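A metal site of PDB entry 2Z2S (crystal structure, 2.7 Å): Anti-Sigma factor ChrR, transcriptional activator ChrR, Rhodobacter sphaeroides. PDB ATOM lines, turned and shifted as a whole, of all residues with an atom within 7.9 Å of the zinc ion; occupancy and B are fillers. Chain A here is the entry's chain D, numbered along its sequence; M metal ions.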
ATOM      1  N   ILE A   3      27.595  -7.610 -10.136  1.00  0.00           N
ATOM      2  CA  ILE A   3      27.119  -8.349 -11.292  1.00  0.00           C
ATOM      3  C   ILE A   3      26.322  -7.503 -12.251  1.00  0.00           C
ATOM      4  O   ILE A   3      25.318  -6.924 -11.864  1.00  0.00           O
ATOM      5  CB  ILE A   3      26.272  -9.527 -10.849  1.00  0.00           C
ATOM      6  CG1 ILE A   3      27.091 -10.390  -9.877  1.00  0.00           C
ATOM      7  CG2 ILE A   3      25.833 -10.331 -12.052  1.00  0.00           C
ATOM      8  CD1 ILE A   3      26.325 -11.485  -9.209  1.00  0.00           C
ATOM      9  N   ARG A   4      26.779  -7.434 -13.500  1.00  0.00           N
ATOM     10  CA  ARG A   4      26.090  -6.637 -14.505  1.00  0.00           C
ATOM     11  C   ARG A   4      25.468  -7.495 -15.597  1.00  0.00           C
ATOM     12  O   ARG A   4      24.642  -7.022 -16.359  1.00  0.00           O
ATOM     13  CB  ARG A   4      27.043  -5.630 -15.151  1.00  0.00           C
ATOM     14  CG  ARG A   4      28.160  -5.143 -14.237  1.00  0.00           C
ATOM     15  CD  ARG A   4      28.936  -3.997 -14.871  1.00  0.00           C
ATOM     16  NE  ARG A   4      30.314  -3.942 -14.364  1.00  0.00           N
ATOM     17  CZ  ARG A   4      30.631  -3.923 -13.075  1.00  0.00           C
ATOM     18  NH1 ARG A   4      29.675  -3.944 -12.167  1.00  0.00           N
ATOM     19  NH2 ARG A   4      31.903  -3.882 -12.694  1.00  0.00           N
ATOM     20  N   HIS A   5      25.855  -8.771 -15.652  1.00  0.00           N
ATOM     21  CA  HIS A   5      25.330  -9.684 -16.672  1.00  0.00           C
ATOM     22  C   HIS A   5      24.523 -10.859 -16.114  1.00  0.00           C
ATOM     23  O   HIS A   5      25.060 -11.784 -15.514  1.00  0.00           O
ATOM     24  CB  HIS A   5      26.488 -10.213 -17.540  1.00  0.00           C
ATOM     25  CG  HIS A   5      27.212  -9.141 -18.280  1.00  0.00           C
ATOM     26  ND1 HIS A   5      28.388  -8.576 -17.827  1.00  0.00           N
ATOM     27  CD2 HIS A   5      26.910  -8.481 -19.422  1.00  0.00           C
ATOM     28  CE1 HIS A   5      28.767  -7.612 -18.652  1.00  0.00           C
ATOM     29  NE2 HIS A   5      27.882  -7.540 -19.630  1.00  0.00           N
ATOM     30  N   HIS A   6      23.224 -10.813 -16.376  1.00  0.00           N
ATOM     31  CA  HIS A   6      22.310 -11.804 -15.854  1.00  0.00           C
ATOM     32  C   HIS A   6      21.763 -12.820 -16.825  1.00  0.00           C
ATOM     33  O   HIS A   6      22.036 -12.776 -18.011  1.00  0.00           O
ATOM     34  CB  HIS A   6      21.156 -11.062 -15.189  1.00  0.00           C
ATOM     35  CG  HIS A   6      21.603 -10.031 -14.199  1.00  0.00           C
ATOM     36  ND1 HIS A   6      22.198 -10.369 -13.001  1.00  0.00           N
ATOM     37  CD2 HIS A   6      21.633  -8.680 -14.261  1.00  0.00           C
ATOM     38  CE1 HIS A   6      22.579  -9.272 -12.372  1.00  0.00           C
ATOM     39  NE2 HIS A   6      22.248  -8.234 -13.118  1.00  0.00           N
ATOM     40  N   VAL A   7      20.983 -13.753 -16.296  1.00  0.00           N
ATOM     41  CA  VAL A   7      20.377 -14.768 -17.103  1.00  0.00           C
ATOM     42  C   VAL A   7      19.155 -14.164 -17.769  1.00  0.00           C
ATOM     43  O   VAL A   7      18.344 -13.479 -17.115  1.00  0.00           O
ATOM     44  CB  VAL A   7      19.944 -15.953 -16.238  1.00  0.00           C
ATOM     45  CG1 VAL A   7      19.378 -17.050 -17.105  1.00  0.00           C
ATOM     46  CG2 VAL A   7      21.136 -16.471 -15.463  1.00  0.00           C
ATOM     47  N   SER A   8      19.026 -14.405 -19.069  1.00  0.00           N
ATOM     48  CA  SER A   8      17.924 -13.873 -19.860  1.00  0.00           C
ATOM     49  C   SER A   8      16.589 -14.284 -19.270  1.00  0.00           C
ATOM     50  O   SER A   8      16.482 -15.320 -18.625  1.00  0.00           O
ATOM     51  CB  SER A   8      18.011 -14.392 -21.279  1.00  0.00           C
ATOM     52  OG  SER A   8      17.870 -15.799 -21.304  1.00  0.00           O
ATOM     53  N   LEU A  12      15.398 -17.851 -17.598  1.00  0.00           N
ATOM     54  CA  LEU A  12      14.799 -17.910 -16.275  1.00  0.00           C
ATOM     55  C   LEU A  12      13.436 -18.546 -16.366  1.00  0.00           C
ATOM     56  O   LEU A  12      13.092 -19.379 -15.540  1.00  0.00           O
ATOM     57  CB  LEU A  12      14.686 -16.521 -15.675  1.00  0.00           C
ATOM     58  CG  LEU A  12      15.667 -16.188 -14.545  1.00  0.00           C
ATOM     59  CD1 LEU A  12      17.073 -16.746 -14.850  1.00  0.00           C
ATOM     60  CD2 LEU A  12      15.701 -14.681 -14.344  1.00  0.00           C
ATOM     61  N   VAL A  28      22.716 -21.666 -14.851  1.00  0.00           N
ATOM     62  CA  VAL A  28      21.721 -20.688 -14.443  1.00  0.00           C
ATOM     63  C   VAL A  28      21.590 -20.694 -12.909  1.00  0.00           C
ATOM     64  O   VAL A  28      21.576 -19.633 -12.271  1.00  0.00           O
ATOM     65  CB  VAL A  28      20.354 -20.984 -15.079  1.00  0.00           C
ATOM     66  CG1 VAL A  28      19.284 -20.098 -14.500  1.00  0.00           C
ATOM     67  CG2 VAL A  28      20.427 -20.782 -16.569  1.00  0.00           C
ATOM     68  N   HIS A  31      24.421 -19.278 -10.906  1.00  0.00           N
ATOM     69  CA  HIS A  31      24.382 -17.828 -10.992  1.00  0.00           C
ATOM     70  C   HIS A  31      23.352 -17.333  -9.986  1.00  0.00           C
ATOM     71  O   HIS A  31      23.626 -16.393  -9.245  1.00  0.00           O
ATOM     72  CB  HIS A  31      23.999 -17.352 -12.397  1.00  0.00           C
ATOM     73  CG  HIS A  31      23.887 -15.872 -12.500  1.00  0.00           C
ATOM     74  ND1 HIS A  31      24.966 -15.032 -12.371  1.00  0.00           N
ATOM     75  CD2 HIS A  31      22.800 -15.063 -12.623  1.00  0.00           C
ATOM     76  CE1 HIS A  31      24.548 -13.771 -12.413  1.00  0.00           C
ATOM     77  NE2 HIS A  31      23.242 -13.771 -12.561  1.00  0.00           N
ATOM     78  N   LEU A  32      22.175 -17.960  -9.943  1.00  0.00           N
ATOM     79  CA  LEU A  32      21.151 -17.549  -8.999  1.00  0.00           C
ATOM     80  C   LEU A  32      21.676 -17.513  -7.571  1.00  0.00           C
ATOM     81  O   LEU A  32      21.300 -16.642  -6.790  1.00  0.00           O
ATOM     82  CB  LEU A  32      19.938 -18.481  -9.064  1.00  0.00           C
ATOM     83  CG  LEU A  32      19.110 -18.385 -10.339  1.00  0.00           C
ATOM     84  CD1 LEU A  32      17.996 -19.417 -10.265  1.00  0.00           C
ATOM     85  CD2 LEU A  32      18.533 -17.014 -10.524  1.00  0.00           C
ATOM     86  N   LEU A  34      24.564 -16.719  -6.673  1.00  0.00           N
ATOM     87  CA  LEU A  34      25.614 -15.713  -6.563  1.00  0.00           C
ATOM     88  C   LEU A  34      25.001 -14.327  -6.778  1.00  0.00           C
ATOM     89  O   LEU A  34      25.545 -13.333  -6.321  1.00  0.00           O
ATOM     90  CB  LEU A  34      26.695 -15.931  -7.623  1.00  0.00           C
ATOM     91  CG  LEU A  34      27.637 -17.148  -7.502  1.00  0.00           C
ATOM     92  CD1 LEU A  34      28.394 -17.328  -8.807  1.00  0.00           C
ATOM     93  CD2 LEU A  34      28.628 -16.958  -6.345  1.00  0.00           C
ATOM     94  N   CYS A  35      23.872 -14.290  -7.466  1.00  0.00           N
ATOM     95  CA  CYS A  35      23.226 -13.042  -7.808  1.00  0.00           C
ATOM     96  C   CYS A  35      21.770 -12.948  -7.318  1.00  0.00           C
ATOM     97  O   CYS A  35      20.859 -13.505  -7.933  1.00  0.00           O
ATOM     98  CB  CYS A  35      23.304 -12.866  -9.323  1.00  0.00           C
ATOM     99  SG  CYS A  35      22.131 -11.741  -9.959  1.00  0.00           S
ATOM    100  N   ASP A  36      21.560 -12.243  -6.203  1.00  0.00           N
ATOM    101  CA  ASP A  36      20.224 -12.075  -5.647  1.00  0.00           C
ATOM    102  C   ASP A  36      19.234 -11.377  -6.593  1.00  0.00           C
ATOM    103  O   ASP A  36      18.039 -11.416  -6.379  1.00  0.00           O
ATOM    104  CB  ASP A  36      20.279 -11.315  -4.323  1.00  0.00           C
ATOM    105  CG  ASP A  36      20.788 -12.173  -3.165  1.00  0.00           C
ATOM    106  OD1 ASP A  36      20.808 -13.415  -3.297  1.00  0.00           O
ATOM    107  OD2 ASP A  36      21.136 -11.599  -2.121  1.00  0.00           O
ATOM    108  N   GLU A  37      19.745 -10.735  -7.631  1.00  0.00           N
ATOM    109  CA  GLU A  37      18.859 -10.065  -8.569  1.00  0.00           C
ATOM    110  C   GLU A  37      18.061 -11.111  -9.352  1.00  0.00           C
ATOM    111  O   GLU A  37      16.827 -11.098  -9.374  1.00  0.00           O
ATOM    112  CB  GLU A  37      19.694  -9.205  -9.517  1.00  0.00           C
ATOM    113  CG  GLU A  37      18.882  -8.417 -10.539  1.00  0.00           C
ATOM    114  CD  GLU A  37      17.707  -7.661  -9.929  1.00  0.00           C
ATOM    115  OE1 GLU A  37      17.851  -7.073  -8.834  1.00  0.00           O
ATOM    116  OE2 GLU A  37      16.651  -7.669 -10.580  1.00  0.00           O
ATOM    117  N   CYS A  38      18.773 -12.014 -10.005  1.00  0.00           N
ATOM    118  CA  CYS A  38      18.139 -13.062 -10.806  1.00  0.00           C
ATOM    119  C   CYS A  38      17.379 -13.987  -9.885  1.00  0.00           C
ATOM    120  O   CYS A  38      16.378 -14.601 -10.259  1.00  0.00           O
ATOM    121  CB  CYS A  38      19.200 -13.838 -11.582  1.00  0.00           C
ATOM    122  SG  CYS A  38      20.204 -12.819 -12.650  1.00  0.00           S
ATOM    123  N   ARG A  39      17.877 -14.096  -8.661  1.00  0.00           N
ATOM    124  CA  ARG A  39      17.234 -14.937  -7.674  1.00  0.00           C
ATOM    125  C   ARG A  39      15.821 -14.408  -7.400  1.00  0.00           C
ATOM    126  O   ARG A  39      14.865 -15.165  -7.223  1.00  0.00           O
ATOM    127  CB  ARG A  39      18.043 -14.924  -6.384  1.00  0.00           C
ATOM    128  CG  ARG A  39      17.557 -15.893  -5.339  1.00  0.00           C
ATOM    129  CD  ARG A  39      18.309 -15.623  -4.032  1.00  0.00           C
ATOM    130  NE  ARG A  39      19.286 -16.653  -3.696  1.00  0.00           N
ATOM    131  CZ  ARG A  39      18.991 -17.947  -3.582  1.00  0.00           C
ATOM    132  NH1 ARG A  39      17.751 -18.373  -3.806  1.00  0.00           N
ATOM    133  NH2 ARG A  39      19.934 -18.791  -3.210  1.00  0.00           N
ATOM    134  N   ARG A  41      14.075 -12.601  -9.587  1.00  0.00           N
ATOM    135  CA  ARG A  41      13.273 -12.699 -10.813  1.00  0.00           C
ATOM    136  C   ARG A  41      12.734 -14.130 -10.953  1.00  0.00           C
ATOM    137  O   ARG A  41      11.569 -14.332 -11.305  1.00  0.00           O
ATOM    138  CB  ARG A  41      14.115 -12.379 -12.028  1.00  0.00           C
ATOM    139  CG  ARG A  41      14.794 -11.052 -11.981  1.00  0.00           C
ATOM    140  CD  ARG A  41      15.603 -10.898 -13.242  1.00  0.00           C
ATOM    141  NE  ARG A  41      16.378  -9.656 -13.304  1.00  0.00           N
ATOM    142  CZ  ARG A  41      17.219  -9.380 -14.293  1.00  0.00           C
ATOM    143  NH1 ARG A  41      17.374 -10.257 -15.291  1.00  0.00           N
ATOM    144  NH2 ARG A  41      17.921  -8.242 -14.289  1.00  0.00           N
ATOM    145  N   GLY A 166      31.030 -14.001 -11.073  1.00  0.00           N
ATOM    146  CA  GLY A 166      29.585 -14.076 -10.977  1.00  0.00           C
ATOM    147  C   GLY A 166      28.810 -13.677 -12.210  1.00  0.00           C
ATOM    148  O   GLY A 166      27.626 -14.015 -12.339  1.00  0.00           O
ATOM    149  N   ASP A 167      29.443 -12.959 -13.132  1.00  0.00           N
ATOM    150  CA  ASP A 167      28.742 -12.529 -14.332  1.00  0.00           C
ATOM    151  C   ASP A 167      28.523 -13.697 -15.307  1.00  0.00           C
ATOM    152  O   ASP A 167      29.333 -14.625 -15.363  1.00  0.00           O
ATOM    153  CB  ASP A 167      29.507 -11.371 -14.993  1.00  0.00           C
ATOM    154  CG  ASP A 167      29.025  -9.988 -14.494  1.00  0.00           C
ATOM    155  OD1 ASP A 167      27.849  -9.640 -14.745  1.00  0.00           O
ATOM    156  OD2 ASP A 167      29.802  -9.248 -13.845  1.00  0.00           O
ATOM    157  N   ILE A 168      27.422 -13.673 -16.037  1.00  0.00           N
ATOM    158  CA  ILE A 168      27.129 -14.745 -16.972  1.00  0.00           C
ATOM    159  C   ILE A 168      26.964 -14.211 -18.384  1.00  0.00           C
ATOM    160  O   ILE A 168      26.388 -13.143 -18.616  1.00  0.00           O
ATOM    161  CB  ILE A 168      25.882 -15.525 -16.544  1.00  0.00           C
ATOM    162  CG1 ILE A 168      25.743 -16.755 -17.433  1.00  0.00           C
ATOM    163  CG2 ILE A 168      24.666 -14.609 -16.567  1.00  0.00           C
ATOM    164  CD1 ILE A 168      24.627 -17.649 -17.064  1.00  0.00           C
HETATM  165 ZN    ZN M   1      21.968 -12.273 -12.404  1.00  0.00          ZN
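The zinc ion is bound by SG of Cys 38, NE2 of His 31, ND1 of His 6 and SG of Cys 35.
The zinc ion has four donor atoms within binding distance.
Of the 20 residues printed, 4 come within 4 Å of the zinc ion.
A ring nitrogen (ND1) of His 31 lies within hydrogen-bond range of the backbone carbonyl oxygen (O) of Gly 166, 2.8 Å away.
The side-chain sulfur (SG) of Cys 35 sits close to the backbone NH (N) of Glu 37.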
